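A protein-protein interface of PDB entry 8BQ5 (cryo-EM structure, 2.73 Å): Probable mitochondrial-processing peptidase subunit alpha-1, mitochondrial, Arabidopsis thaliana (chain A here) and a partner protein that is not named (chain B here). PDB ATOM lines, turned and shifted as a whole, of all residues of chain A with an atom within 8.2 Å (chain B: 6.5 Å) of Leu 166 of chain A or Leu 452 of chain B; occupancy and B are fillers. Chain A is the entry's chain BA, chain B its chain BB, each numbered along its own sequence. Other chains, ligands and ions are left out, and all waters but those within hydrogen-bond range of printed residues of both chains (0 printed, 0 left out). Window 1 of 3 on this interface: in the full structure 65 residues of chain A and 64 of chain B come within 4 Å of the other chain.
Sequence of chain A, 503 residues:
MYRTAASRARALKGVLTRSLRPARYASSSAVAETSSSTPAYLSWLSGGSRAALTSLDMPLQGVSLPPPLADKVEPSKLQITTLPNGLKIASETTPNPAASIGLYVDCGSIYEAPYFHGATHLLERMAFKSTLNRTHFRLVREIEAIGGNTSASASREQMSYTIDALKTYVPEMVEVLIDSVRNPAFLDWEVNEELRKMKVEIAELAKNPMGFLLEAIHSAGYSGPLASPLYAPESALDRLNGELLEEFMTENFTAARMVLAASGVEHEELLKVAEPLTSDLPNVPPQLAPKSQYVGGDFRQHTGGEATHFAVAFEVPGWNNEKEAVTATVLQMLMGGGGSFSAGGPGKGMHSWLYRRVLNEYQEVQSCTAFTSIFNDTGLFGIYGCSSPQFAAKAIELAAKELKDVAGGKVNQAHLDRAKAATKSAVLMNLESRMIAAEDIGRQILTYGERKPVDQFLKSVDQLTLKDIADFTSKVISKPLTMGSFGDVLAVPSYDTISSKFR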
ATOM      1  N   ASN A  96     -28.255 -37.000  -1.714  1.00  0.00           N
ATOM      2  CA  ASN A  96     -28.810 -36.417  -0.502  1.00  0.00           C
ATOM      3  C   ASN A  96     -29.353 -35.018  -0.793  1.00  0.00           C
ATOM      4  O   ASN A  96     -28.672 -34.207  -1.430  1.00  0.00           O
ATOM      5  CB  ASN A  96     -27.735 -36.367   0.586  1.00  0.00           C
ATOM      6  CG  ASN A  96     -28.045 -35.371   1.684  1.00  0.00           C
ATOM      7  OD1 ASN A  96     -29.150 -35.340   2.224  1.00  0.00           O
ATOM      8  ND2 ASN A  96     -27.058 -34.555   2.032  1.00  0.00           N
ATOM      9  N   PRO A  97     -30.579 -34.713  -0.362  1.00  0.00           N
ATOM     10  CA  PRO A  97     -31.161 -33.395  -0.667  1.00  0.00           C
ATOM     11  C   PRO A  97     -30.407 -32.221  -0.066  1.00  0.00           C
ATOM     12  O   PRO A  97     -30.566 -31.095  -0.551  1.00  0.00           O
ATOM     13  CB  PRO A  97     -32.582 -33.497  -0.091  1.00  0.00           C
ATOM     14  CG  PRO A  97     -32.513 -34.618   0.897  1.00  0.00           C
ATOM     15  CD  PRO A  97     -31.553 -35.594   0.303  1.00  0.00           C
ATOM     16  N   ALA A  98     -29.610 -32.430   0.976  1.00  0.00           N
ATOM     17  CA  ALA A  98     -28.855 -31.338   1.573  1.00  0.00           C
ATOM     18  C   ALA A  98     -27.635 -31.006   0.724  1.00  0.00           C
ATOM     19  O   ALA A  98     -27.063 -31.875   0.061  1.00  0.00           O
ATOM     20  CB  ALA A  98     -28.425 -31.694   2.994  1.00  0.00           C
ATOM     21  N   ALA A  99     -27.238 -29.737   0.750  1.00  0.00           N
ATOM     22  CA  ALA A  99     -26.064 -29.264   0.035  1.00  0.00           C
ATOM     23  C   ALA A  99     -25.125 -28.561   1.003  1.00  0.00           C
ATOM     24  O   ALA A  99     -25.559 -27.966   1.994  1.00  0.00           O
ATOM     25  CB  ALA A  99     -26.445 -28.316  -1.107  1.00  0.00           C
ATOM     26  N   SER A 100     -23.829 -28.640   0.710  1.00  0.00           N
ATOM     27  CA  SER A 100     -22.795 -28.049   1.548  1.00  0.00           C
ATOM     28  C   SER A 100     -21.775 -27.365   0.653  1.00  0.00           C
ATOM     29  O   SER A 100     -21.071 -28.034  -0.110  1.00  0.00           O
ATOM     30  CB  SER A 100     -22.120 -29.112   2.421  1.00  0.00           C
ATOM     31  OG  SER A 100     -21.353 -28.518   3.453  1.00  0.00           O
ATOM     32  N   ILE A 101     -21.698 -26.041   0.745  1.00  0.00           N
ATOM     33  CA  ILE A 101     -20.763 -25.242  -0.038  1.00  0.00           C
ATOM     34  C   ILE A 101     -19.832 -24.515   0.921  1.00  0.00           C
ATOM     35  O   ILE A 101     -20.292 -23.840   1.849  1.00  0.00           O
ATOM     36  CB  ILE A 101     -21.492 -24.245  -0.955  1.00  0.00           C
ATOM     37  CG1 ILE A 101     -22.608 -24.954  -1.723  1.00  0.00           C
ATOM     38  CG2 ILE A 101     -20.509 -23.582  -1.907  1.00  0.00           C
ATOM     39  CD1 ILE A 101     -23.328 -24.072  -2.713  1.00  0.00           C
ATOM     40  N   ILE A 146     -33.848 -19.318   3.862  1.00  0.00           N
ATOM     41  CA  ILE A 146     -33.655 -20.579   3.157  1.00  0.00           C
ATOM     42  C   ILE A 146     -33.394 -21.732   4.119  1.00  0.00           C
ATOM     43  O   ILE A 146     -33.155 -22.860   3.678  1.00  0.00           O
ATOM     44  CB  ILE A 146     -32.526 -20.464   2.119  1.00  0.00           C
ATOM     45  CG1 ILE A 146     -31.211 -20.076   2.795  1.00  0.00           C
ATOM     46  CG2 ILE A 146     -32.889 -19.451   1.048  1.00  0.00           C
ATOM     47  CD1 ILE A 146     -30.006 -20.798   2.244  1.00  0.00           C
ATOM     48  N   GLY A 147     -33.437 -21.477   5.425  1.00  0.00           N
ATOM     49  CA  GLY A 147     -33.214 -22.528   6.403  1.00  0.00           C
ATOM     50  C   GLY A 147     -31.775 -22.974   6.513  1.00  0.00           C
ATOM     51  O   GLY A 147     -31.506 -24.063   7.029  1.00  0.00           O
ATOM     52  N   GLY A 148     -30.832 -22.152   6.049  1.00  0.00           N
ATOM     53  CA  GLY A 148     -29.440 -22.541   6.030  1.00  0.00           C
ATOM     54  C   GLY A 148     -28.733 -22.343   7.360  1.00  0.00           C
ATOM     55  O   GLY A 148     -29.283 -21.805   8.319  1.00  0.00           O
ATOM     56  N   ASN A 149     -27.486 -22.807   7.402  1.00  0.00           N
ATOM     57  CA  ASN A 149     -26.604 -22.630   8.547  1.00  0.00           C
ATOM     58  C   ASN A 149     -25.215 -22.260   8.052  1.00  0.00           C
ATOM     59  O   ASN A 149     -24.758 -22.768   7.025  1.00  0.00           O
ATOM     60  CB  ASN A 149     -26.525 -23.897   9.407  1.00  0.00           C
ATOM     61  CG  ASN A 149     -27.889 -24.403   9.824  1.00  0.00           C
ATOM     62  OD1 ASN A 149     -28.479 -25.251   9.156  1.00  0.00           O
ATOM     63  ND2 ASN A 149     -28.396 -23.887  10.937  1.00  0.00           N
ATOM     64  N   THR A 150     -24.547 -21.383   8.791  1.00  0.00           N
ATOM     65  CA  THR A 150     -23.214 -20.919   8.441  1.00  0.00           C
ATOM     66  C   THR A 150     -22.223 -21.299   9.531  1.00  0.00           C
ATOM     67  O   THR A 150     -22.570 -21.415  10.710  1.00  0.00           O
ATOM     68  CB  THR A 150     -23.198 -19.402   8.227  1.00  0.00           C
ATOM     69  OG1 THR A 150     -23.879 -18.759   9.311  1.00  0.00           O
ATOM     70  CG2 THR A 150     -23.886 -19.048   6.922  1.00  0.00           C
ATOM     71  N   ILE A 163     -21.502 -22.976   4.195  1.00  0.00           N
ATOM     72  CA  ILE A 163     -22.948 -22.808   4.294  1.00  0.00           C
ATOM     73  C   ILE A 163     -23.603 -24.148   3.990  1.00  0.00           C
ATOM     74  O   ILE A 163     -23.273 -24.791   2.986  1.00  0.00           O
ATOM     75  CB  ILE A 163     -23.473 -21.723   3.335  1.00  0.00           C
ATOM     76  CG1 ILE A 163     -22.649 -20.441   3.460  1.00  0.00           C
ATOM     77  CG2 ILE A 163     -24.946 -21.447   3.602  1.00  0.00           C
ATOM     78  CD1 ILE A 163     -23.338 -19.219   2.896  1.00  0.00           C
ATOM     79  N   ASP A 164     -24.529 -24.566   4.850  1.00  0.00           N
ATOM     80  CA  ASP A 164     -25.292 -25.794   4.660  1.00  0.00           C
ATOM     81  C   ASP A 164     -26.764 -25.451   4.504  1.00  0.00           C
ATOM     82  O   ASP A 164     -27.327 -24.738   5.340  1.00  0.00           O
ATOM     83  CB  ASP A 164     -25.109 -26.756   5.837  1.00  0.00           C
ATOM     84  CG  ASP A 164     -23.658 -27.096   6.095  1.00  0.00           C
ATOM     85  OD1 ASP A 164     -22.896 -27.252   5.117  1.00  0.00           O
ATOM     86  OD2 ASP A 164     -23.279 -27.208   7.279  1.00  0.00           O
ATOM     87  N   ALA A 165     -27.384 -25.967   3.448  1.00  0.00           N
ATOM     88  CA  ALA A 165     -28.807 -25.762   3.206  1.00  0.00           C
ATOM     89  C   ALA A 165     -29.279 -26.812   2.209  1.00  0.00           C
ATOM     90  O   ALA A 165     -28.515 -27.685   1.788  1.00  0.00           O
ATOM     91  CB  ALA A 165     -29.089 -24.344   2.702  1.00  0.00           C
ATOM     92  N   LEU A 166     -30.550 -26.719   1.831  1.00  0.00           N
ATOM     93  CA  LEU A 166     -31.112 -27.645   0.860  1.00  0.00           C
ATOM     94  C   LEU A 166     -30.533 -27.381  -0.525  1.00  0.00           C
ATOM     95  O   LEU A 166     -29.967 -26.319  -0.798  1.00  0.00           O
ATOM     96  CB  LEU A 166     -32.634 -27.529   0.827  1.00  0.00           C
ATOM     97  CG  LEU A 166     -33.404 -28.121   2.011  1.00  0.00           C
ATOM     98  CD1 LEU A 166     -34.875 -28.272   1.665  1.00  0.00           C
ATOM     99  CD2 LEU A 166     -32.815 -29.457   2.436  1.00  0.00           C
ATOM    100  N   LYS A 167     -30.684 -28.370  -1.409  1.00  0.00           N
ATOM    101  CA  LYS A 167     -30.052 -28.311  -2.723  1.00  0.00           C
ATOM    102  C   LYS A 167     -30.701 -27.290  -3.649  1.00  0.00           C
ATOM    103  O   LYS A 167     -30.057 -26.847  -4.605  1.00  0.00           O
ATOM    104  CB  LYS A 167     -30.084 -29.691  -3.379  1.00  0.00           C
ATOM    105  CG  LYS A 167     -28.812 -30.494  -3.166  1.00  0.00           C
ATOM    106  CD  LYS A 167     -28.919 -31.918  -3.706  1.00  0.00           C
ATOM    107  CE  LYS A 167     -30.078 -32.093  -4.671  1.00  0.00           C
ATOM    108  NZ  LYS A 167     -29.992 -33.396  -5.383  1.00  0.00           N
ATOM    109  N   THR A 168     -31.952 -26.908  -3.395  1.00  0.00           N
ATOM    110  CA  THR A 168     -32.639 -25.973  -4.277  1.00  0.00           C
ATOM    111  C   THR A 168     -32.192 -24.531  -4.076  1.00  0.00           C
ATOM    112  O   THR A 168     -32.594 -23.664  -4.859  1.00  0.00           O
ATOM    113  CB  THR A 168     -34.151 -26.074  -4.074  1.00  0.00           C
ATOM    114  OG1 THR A 168     -34.472 -25.809  -2.704  1.00  0.00           O
ATOM    115  CG2 THR A 168     -34.641 -27.463  -4.442  1.00  0.00           C
ATOM    116  N   TYR A 169     -31.376 -24.254  -3.060  1.00  0.00           N
ATOM    117  CA  TYR A 169     -30.952 -22.897  -2.740  1.00  0.00           C
ATOM    118  C   TYR A 169     -29.479 -22.657  -3.042  1.00  0.00           C
ATOM    119  O   TYR A 169     -28.838 -21.843  -2.372  1.00  0.00           O
ATOM    120  CB  TYR A 169     -31.244 -22.591  -1.272  1.00  0.00           C
ATOM    121  CG  TYR A 169     -32.698 -22.743  -0.904  1.00  0.00           C
ATOM    122  CD1 TYR A 169     -33.664 -21.926  -1.472  1.00  0.00           C
ATOM    123  CD2 TYR A 169     -33.106 -23.706   0.008  1.00  0.00           C
ATOM    124  CE1 TYR A 169     -34.994 -22.060  -1.140  1.00  0.00           C
ATOM    125  CE2 TYR A 169     -34.435 -23.848   0.345  1.00  0.00           C
ATOM    126  CZ  TYR A 169     -35.374 -23.022  -0.231  1.00  0.00           C
ATOM    127  OH  TYR A 169     -36.701 -23.158   0.101  1.00  0.00           O
ATOM    128  N   VAL A 170     -28.929 -23.353  -4.036  1.00  0.00           N
ATOM    129  CA  VAL A 170     -27.510 -23.194  -4.361  1.00  0.00           C
ATOM    130  C   VAL A 170     -27.158 -21.769  -4.786  1.00  0.00           C
ATOM    131  O   VAL A 170     -26.166 -21.229  -4.277  1.00  0.00           O
ATOM    132  CB  VAL A 170     -27.085 -24.248  -5.397  1.00  0.00           C
ATOM    133  CG1 VAL A 170     -25.745 -23.883  -6.016  1.00  0.00           C
ATOM    134  CG2 VAL A 170     -27.023 -25.615  -4.745  1.00  0.00           C
ATOM    135  N   PRO A 171     -27.897 -21.113  -5.693  1.00  0.00           N
ATOM    136  CA  PRO A 171     -27.509 -19.739  -6.067  1.00  0.00           C
ATOM    137  C   PRO A 171     -27.512 -18.765  -4.900  1.00  0.00           C
ATOM    138  O   PRO A 171     -26.681 -17.851  -4.862  1.00  0.00           O
ATOM    139  CB  PRO A 171     -28.547 -19.357  -7.133  1.00  0.00           C
ATOM    140  CG  PRO A 171     -29.085 -20.646  -7.628  1.00  0.00           C
ATOM    141  CD  PRO A 171     -29.080 -21.558  -6.452  1.00  0.00           C
ATOM    142  N   GLU A 172     -28.427 -18.934  -3.944  1.00  0.00           N
ATOM    143  CA  GLU A 172     -28.463 -18.032  -2.798  1.00  0.00           C
ATOM    144  C   GLU A 172     -27.309 -18.297  -1.841  1.00  0.00           C
ATOM    145  O   GLU A 172     -26.745 -17.359  -1.266  1.00  0.00           O
ATOM    146  CB  GLU A 172     -29.805 -18.154  -2.077  1.00  0.00           C
ATOM    147  CG  GLU A 172     -30.983 -17.660  -2.898  1.00  0.00           C
ATOM    148  CD  GLU A 172     -31.903 -18.776  -3.340  1.00  0.00           C
ATOM    149  OE1 GLU A 172     -31.399 -19.803  -3.838  1.00  0.00           O
ATOM    150  OE2 GLU A 172     -33.133 -18.622  -3.196  1.00  0.00           O
ATOM    151  N   MET A 173     -26.946 -19.567  -1.649  1.00  0.00           N
ATOM    152  CA  MET A 173     -25.840 -19.892  -0.753  1.00  0.00           C
ATOM    153  C   MET A 173     -24.521 -19.354  -1.293  1.00  0.00           C
ATOM    154  O   MET A 173     -23.679 -18.864  -0.534  1.00  0.00           O
ATOM    155  CB  MET A 173     -25.753 -21.405  -0.542  1.00  0.00           C
ATOM    156  CG  MET A 173     -26.956 -22.019   0.148  1.00  0.00           C
ATOM    157  SD  MET A 173     -27.132 -23.775  -0.225  1.00  0.00           S
ATOM    158  CE  MET A 173     -25.664 -24.442   0.553  1.00  0.00           C
ATOM    159  N   GLY A 264     -22.784 -31.771  -3.163  1.00  0.00           N
ATOM    160  CA  GLY A 264     -24.217 -31.866  -3.352  1.00  0.00           C
ATOM    161  C   GLY A 264     -24.767 -30.988  -4.457  1.00  0.00           C
ATOM    162  O   GLY A 264     -25.984 -30.820  -4.565  1.00  0.00           O
ATOM    163  N   VAL A 265     -23.892 -30.418  -5.281  1.00  0.00           N
ATOM    164  CA  VAL A 265     -24.311 -29.566  -6.388  1.00  0.00           C
ATOM    165  C   VAL A 265     -23.677 -30.085  -7.671  1.00  0.00           C
ATOM    166  O   VAL A 265     -22.681 -30.815  -7.644  1.00  0.00           O
ATOM    167  CB  VAL A 265     -23.935 -28.081  -6.166  1.00  0.00           C
ATOM    168  CG1 VAL A 265     -24.118 -27.688  -4.710  1.00  0.00           C
ATOM    169  CG2 VAL A 265     -22.512 -27.810  -6.622  1.00  0.00           C
ATOM    170  N   SER A 433     -20.527 -38.268   6.542  1.00  0.00           N
ATOM    171  CA  SER A 433     -21.137 -36.972   6.801  1.00  0.00           C
ATOM    172  C   SER A 433     -20.775 -36.005   5.680  1.00  0.00           C
ATOM    173  O   SER A 433     -19.597 -35.838   5.347  1.00  0.00           O
ATOM    174  CB  SER A 433     -20.670 -36.427   8.149  1.00  0.00           C
ATOM    175  OG  SER A 433     -21.072 -35.081   8.321  1.00  0.00           O
ATOM    176  N   ARG A 434     -21.791 -35.365   5.096  1.00  0.00           N
ATOM    177  CA  ARG A 434     -21.558 -34.526   3.925  1.00  0.00           C
ATOM    178  C   ARG A 434     -20.711 -33.303   4.266  1.00  0.00           C
ATOM    179  O   ARG A 434     -19.955 -32.811   3.421  1.00  0.00           O
ATOM    180  CB  ARG A 434     -22.890 -34.100   3.306  1.00  0.00           C
ATOM    181  CG  ARG A 434     -23.578 -33.002   4.080  1.00  0.00           C
ATOM    182  CD  ARG A 434     -24.767 -32.408   3.357  1.00  0.00           C
ATOM    183  NE  ARG A 434     -25.257 -31.239   4.077  1.00  0.00           N
ATOM    184  CZ  ARG A 434     -25.769 -31.268   5.302  1.00  0.00           C
ATOM    185  NH1 ARG A 434     -25.988 -32.408   5.937  1.00  0.00           N
ATOM    186  NH2 ARG A 434     -26.076 -30.122   5.902  1.00  0.00           N
ATOM    187  N   MET A 435     -20.829 -32.792   5.495  1.00  0.00           N
ATOM    188  CA  MET A 435     -20.045 -31.619   5.875  1.00  0.00           C
ATOM    189  C   MET A 435     -18.558 -31.944   5.930  1.00  0.00           C
ATOM    190  O   MET A 435     -17.726 -31.133   5.508  1.00  0.00           O
ATOM    191  CB  MET A 435     -20.528 -31.068   7.216  1.00  0.00           C
ATOM    192  CG  MET A 435     -22.023 -30.819   7.286  1.00  0.00           C
ATOM    193  SD  MET A 435     -22.614 -30.665   8.981  1.00  0.00           S
ATOM    194  CE  MET A 435     -23.510 -32.202   9.170  1.00  0.00           C
ATOM    195  N   ILE B  91     -36.270 -33.095  -5.341  1.00  0.00           N
ATOM    196  CA  ILE B  91     -35.009 -33.321  -4.643  1.00  0.00           C
ATOM    197  C   ILE B  91     -35.274 -34.155  -3.397  1.00  0.00           C
ATOM    198  O   ILE B  91     -34.348 -34.484  -2.647  1.00  0.00           O
ATOM    199  CB  ILE B  91     -34.320 -31.993  -4.282  1.00  0.00           C
ATOM    200  CG1 ILE B  91     -35.264 -31.101  -3.473  1.00  0.00           C
ATOM    201  CG2 ILE B  91     -33.858 -31.275  -5.538  1.00  0.00           C
ATOM    202  CD1 ILE B  91     -34.636 -30.526  -2.223  1.00  0.00           C
ATOM    203  N   LEU B  92     -36.538 -34.505  -3.173  1.00  0.00           N
ATOM    204  CA  LEU B  92     -36.938 -35.231  -1.977  1.00  0.00           C
ATOM    205  C   LEU B  92     -36.815 -36.741  -2.124  1.00  0.00           C
ATOM    206  O   LEU B  92     -37.109 -37.465  -1.167  1.00  0.00           O
ATOM    207  CB  LEU B  92     -38.376 -34.860  -1.608  1.00  0.00           C
ATOM    208  CG  LEU B  92     -38.596 -34.444  -0.155  1.00  0.00           C
ATOM    209  CD1 LEU B  92     -37.569 -33.405   0.259  1.00  0.00           C
ATOM    210  CD2 LEU B  92     -40.003 -33.909   0.038  1.00  0.00           C
ATOM    211  N   ASN B 444     -39.714 -23.236   6.921  1.00  0.00           N
ATOM    212  CA  ASN B 444     -38.514 -23.447   6.118  1.00  0.00           C
ATOM    213  C   ASN B 444     -37.358 -23.943   6.973  1.00  0.00           C
ATOM    214  O   ASN B 444     -36.595 -24.820   6.552  1.00  0.00           O
ATOM    215  CB  ASN B 444     -38.133 -22.154   5.399  1.00  0.00           C
ATOM    216  CG  ASN B 444     -39.068 -21.829   4.258  1.00  0.00           C
ATOM    217  OD1 ASN B 444     -39.877 -22.659   3.848  1.00  0.00           O
ATOM    218  ND2 ASN B 444     -38.968 -20.611   3.740  1.00  0.00           N
ATOM    219  N   LYS B 447     -38.112 -27.728   8.078  1.00  0.00           N
ATOM    220  CA  LYS B 447     -37.897 -28.676   6.990  1.00  0.00           C
ATOM    221  C   LYS B 447     -36.412 -28.880   6.729  1.00  0.00           C
ATOM    222  O   LYS B 447     -35.956 -30.008   6.505  1.00  0.00           O
ATOM    223  CB  LYS B 447     -38.599 -28.191   5.722  1.00  0.00           C
ATOM    224  CG  LYS B 447     -40.106 -28.138   5.824  1.00  0.00           C
ATOM    225  CD  LYS B 447     -40.744 -28.172   4.449  1.00  0.00           C
ATOM    226  CE  LYS B 447     -41.216 -26.794   4.027  1.00  0.00           C
ATOM    227  NZ  LYS B 447     -42.244 -26.875   2.955  1.00  0.00           N
ATOM    228  N   SER B 448     -35.641 -27.792   6.744  1.00  0.00           N
ATOM    229  CA  SER B 448     -34.207 -27.896   6.501  1.00  0.00           C
ATOM    230  C   SER B 448     -33.511 -28.683   7.603  1.00  0.00           C
ATOM    231  O   SER B 448     -32.671 -29.546   7.324  1.00  0.00           O
ATOM    232  CB  SER B 448     -33.597 -26.502   6.373  1.00  0.00           C
ATOM    233  OG  SER B 448     -32.193 -26.574   6.203  1.00  0.00           O
ATOM    234  N   SER B 449     -33.849 -28.404   8.865  1.00  0.00           N
ATOM    235  CA  SER B 449     -33.159 -29.053   9.974  1.00  0.00           C
ATOM    236  C   SER B 449     -33.474 -30.541  10.045  1.00  0.00           C
ATOM    237  O   SER B 449     -32.601 -31.338  10.407  1.00  0.00           O
ATOM    238  CB  SER B 449     -33.520 -28.370  11.294  1.00  0.00           C
ATOM    239  OG  SER B 449     -34.824 -28.724  11.717  1.00  0.00           O
ATOM    240  N   LEU B 450     -34.706 -30.936   9.715  1.00  0.00           N
ATOM    241  CA  LEU B 450     -35.042 -32.355   9.700  1.00  0.00           C
ATOM    242  C   LEU B 450     -34.287 -33.097   8.606  1.00  0.00           C
ATOM    243  O   LEU B 450     -33.940 -34.270   8.780  1.00  0.00           O
ATOM    244  CB  LEU B 450     -36.547 -32.545   9.518  1.00  0.00           C
ATOM    245  CG  LEU B 450     -37.451 -32.113  10.671  1.00  0.00           C
ATOM    246  CD1 LEU B 450     -38.906 -32.152  10.238  1.00  0.00           C
ATOM    247  CD2 LEU B 450     -37.228 -32.990  11.888  1.00  0.00           C
ATOM    248  N   LEU B 451     -34.030 -32.438   7.481  1.00  0.00           N
ATOM    249  CA  LEU B 451     -33.348 -33.067   6.360  1.00  0.00           C
ATOM    250  C   LEU B 451     -31.832 -32.941   6.434  1.00  0.00           C
ATOM    251  O   LEU B 451     -31.127 -33.837   5.956  1.00  0.00           O
ATOM    252  CB  LEU B 451     -33.844 -32.459   5.046  1.00  0.00           C
ATOM    253  CG  LEU B 451     -34.222 -33.423   3.923  1.00  0.00           C
ATOM    254  CD1 LEU B 451     -35.046 -34.577   4.459  1.00  0.00           C
ATOM    255  CD2 LEU B 451     -34.990 -32.678   2.850  1.00  0.00           C
ATOM    256  N   LEU B 452     -31.317 -31.857   7.017  1.00  0.00           N
ATOM    257  CA  LEU B 452     -29.875 -31.651   7.086  1.00  0.00           C
ATOM    258  C   LEU B 452     -29.199 -32.637   8.028  1.00  0.00           C
ATOM    259  O   LEU B 452     -28.065 -33.057   7.768  1.00  0.00           O
ATOM    260  CB  LEU B 452     -29.572 -30.218   7.526  1.00  0.00           C
ATOM    261  CG  LEU B 452     -29.127 -29.228   6.445  1.00  0.00           C
ATOM    262  CD1 LEU B 452     -30.024 -29.310   5.220  1.00  0.00           C
ATOM    263  CD2 LEU B 452     -29.098 -27.812   6.995  1.00  0.00           C
ATOM    264  N   HIS B 453     -29.865 -33.013   9.119  1.00  0.00           N
ATOM    265  CA  HIS B 453     -29.300 -33.961  10.070  1.00  0.00           C
ATOM    266  C   HIS B 453     -29.475 -35.413   9.637  1.00  0.00           C
ATOM    267  O   HIS B 453     -28.964 -36.309  10.316  1.00  0.00           O
ATOM    268  CB  HIS B 453     -29.912 -33.729  11.453  1.00  0.00           C
ATOM    269  CG  HIS B 453     -29.673 -32.360  12.006  1.00  0.00           C
ATOM    270  ND1 HIS B 453     -28.426 -31.925  12.401  1.00  0.00           N
ATOM    271  CD2 HIS B 453     -30.522 -31.332  12.241  1.00  0.00           C
ATOM    272  CE1 HIS B 453     -28.518 -30.689  12.857  1.00  0.00           C
ATOM    273  NE2 HIS B 453     -29.779 -30.305  12.769  1.00  0.00           N
ATOM    274  N   MET B 454     -30.162 -35.661   8.525  1.00  0.00           N
ATOM    275  CA  MET B 454     -30.308 -37.005   7.964  1.00  0.00           C
ATOM    276  C   MET B 454     -29.093 -37.403   7.130  1.00  0.00           C
ATOM    277  O   MET B 454     -29.219 -37.785   5.967  1.00  0.00           O
ATOM    278  CB  MET B 454     -31.581 -37.082   7.131  1.00  0.00           C
ATOM    279  CG  MET B 454     -32.860 -37.172   7.933  1.00  0.00           C
ATOM    280  SD  MET B 454     -33.099 -38.808   8.648  1.00  0.00           S
ATOM    281  CE  MET B 454     -32.774 -38.476  10.367  1.00  0.00           C
ATOM    282  N   ASP B 455     -27.900 -37.311   7.710  1.00  0.00           N
ATOM    283  CA  ASP B 455     -26.681 -37.724   7.029  1.00  0.00           C
ATOM    284  C   ASP B 455     -25.918 -38.695   7.915  1.00  0.00           C
ATOM    285  O   ASP B 455     -25.774 -38.463   9.119  1.00  0.00           O
ATOM    286  CB  ASP B 455     -25.799 -36.522   6.666  1.00  0.00           C
ATOM    287  CG  ASP B 455     -25.466 -35.656   7.861  1.00  0.00           C
ATOM    288  OD1 ASP B 455     -26.180 -35.735   8.882  1.00  0.00           O
ATOM    289  OD2 ASP B 455     -24.482 -34.893   7.776  1.00  0.00           O
ATOM    290  N   PHE B 481     -43.399 -33.040   5.033  1.00  0.00           N
ATOM    291  CA  PHE B 481     -43.380 -31.676   4.518  1.00  0.00           C
ATOM    292  C   PHE B 481     -44.792 -31.149   4.304  1.00  0.00           C
ATOM    293  O   PHE B 481     -45.070 -29.973   4.564  1.00  0.00           O
ATOM    294  CB  PHE B 481     -42.581 -31.621   3.216  1.00  0.00           C
ATOM    295  CG  PHE B 481     -41.098 -31.507   3.418  1.00  0.00           C
ATOM    296  CD1 PHE B 481     -40.514 -31.914   4.606  1.00  0.00           C
ATOM    297  CD2 PHE B 481     -40.289 -30.996   2.420  1.00  0.00           C
ATOM    298  CE1 PHE B 481     -39.152 -31.811   4.793  1.00  0.00           C
ATOM    299  CE2 PHE B 481     -38.926 -30.889   2.604  1.00  0.00           C
ATOM    300  CZ  PHE B 481     -38.358 -31.298   3.791  1.00  0.00           C
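The side-chain amide oxygen (OD1) of Asn 96 of chain A lies close to the backbone NH (N) of Ala 98 of chain A (3.2 Å).
O of Pro 97 of chain A lies within hydrogen-bond range of N of Lys 167 of chain A (2.9 Å).
O of Ala 165 of chain A lies within hydrogen-bond range of N of Ala 99 of chain A, 2.6 Å away.
OG of Ser 100 of chain A is in hydrogen-bond range of OD1 of Asp 164 of chain A (2.6 Å).
N of Asn 149 of chain A sits at hydrogen-bond distance from O of Asp 164 of chain A, at 2.8 Å.
Printed residues of chain A that touch a printed residue of chain B: Pro 97, Ala 98, Gly 147, Asn 149, Asp 164, Ala 165, Leu 166, Lys 167, Thr 168, Ser 433, Arg 434 and Met 435.
Hydrophobic or aromatic side chains of chain A within 4 Å of the printed part of chain B: Pro 97, Ala 98, Leu 166 and Met 435.
Along chain A the printed residues that touch a printed residue of chain B span positions 97 to 435.
Of the 13 printed residues of chain B, 5 touch a printed residue of chain A.
Printed residues of chain B within 4 Å of Pro 97 of chain A: Ile 91 and Leu 451.
Thr 150 of chain A touches none of the printed residues of chain B.
Ile 163 of chain A touches none of the printed residues of chain B.
Of the printed residues of chain A, Ile 91 of chain B touches Pro 97, Lys 167 and Thr 168.
Printed residues of chain A within 4 Å of Leu 452 of chain B: Ala 98 (3.6 Å), Asn 149 (3.4 Å), Asp 164 (3.9 Å), Ala 165 (3.98 Å), Leu 166 (3.9 Å) and Arg 434 (2.8 Å).
The nearest residue of chain B that does not touch Leu 166 of chain A is Ile 91 of chain B (4.5 Å).
The nearest printed residue of chain A that does not touch Leu 452 of chain B is Gly 147 of chain A (4.5 Å).
CG of Pro 97 of chain A touches CG of Leu 451 of chain B, at 3.7 Å.
Ala 98 of chain A touches Leu 452 of chain B.
CD2 of Leu 452 of chain B touches O of Asp 164 of chain A, 3.9 Å away.
CD1 of Leu 452 of chain B touches C of Ala 165 of chain A (3.98 Å).
Leu 166 of chain A touches Leu 451 of chain B (CD2 to CD2, 3.9 Å).
Thr 168 of chain A touches Ile 91 of chain B (CG2 to CD1, 3.8 Å).
Met 435 of chain A touches Asp 455 of chain B (CE to OD2, 3.2 Å).
The backbone carbonyl oxygen of Gly 147 of chain A is in hydrogen-bond range of the side-chain hydroxyl of Ser 448 of chain B, 2.7 Å away.
The side-chain hydroxyl (OG) of Ser 433 of chain A lies within hydrogen-bond range of the side-chain carboxylate (OD2) of Asp 455 of chain B (3.5 Å).
O of Leu 452 of chain B sits at hydrogen-bond distance from NH1 of Arg 434 of chain A.
The side-chain carboxylate (OD2) of Asp 455 of chain B lies within salt-bridge range of the guanidinium group (NH1) of Arg 434 of chain A (3.4 Å).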
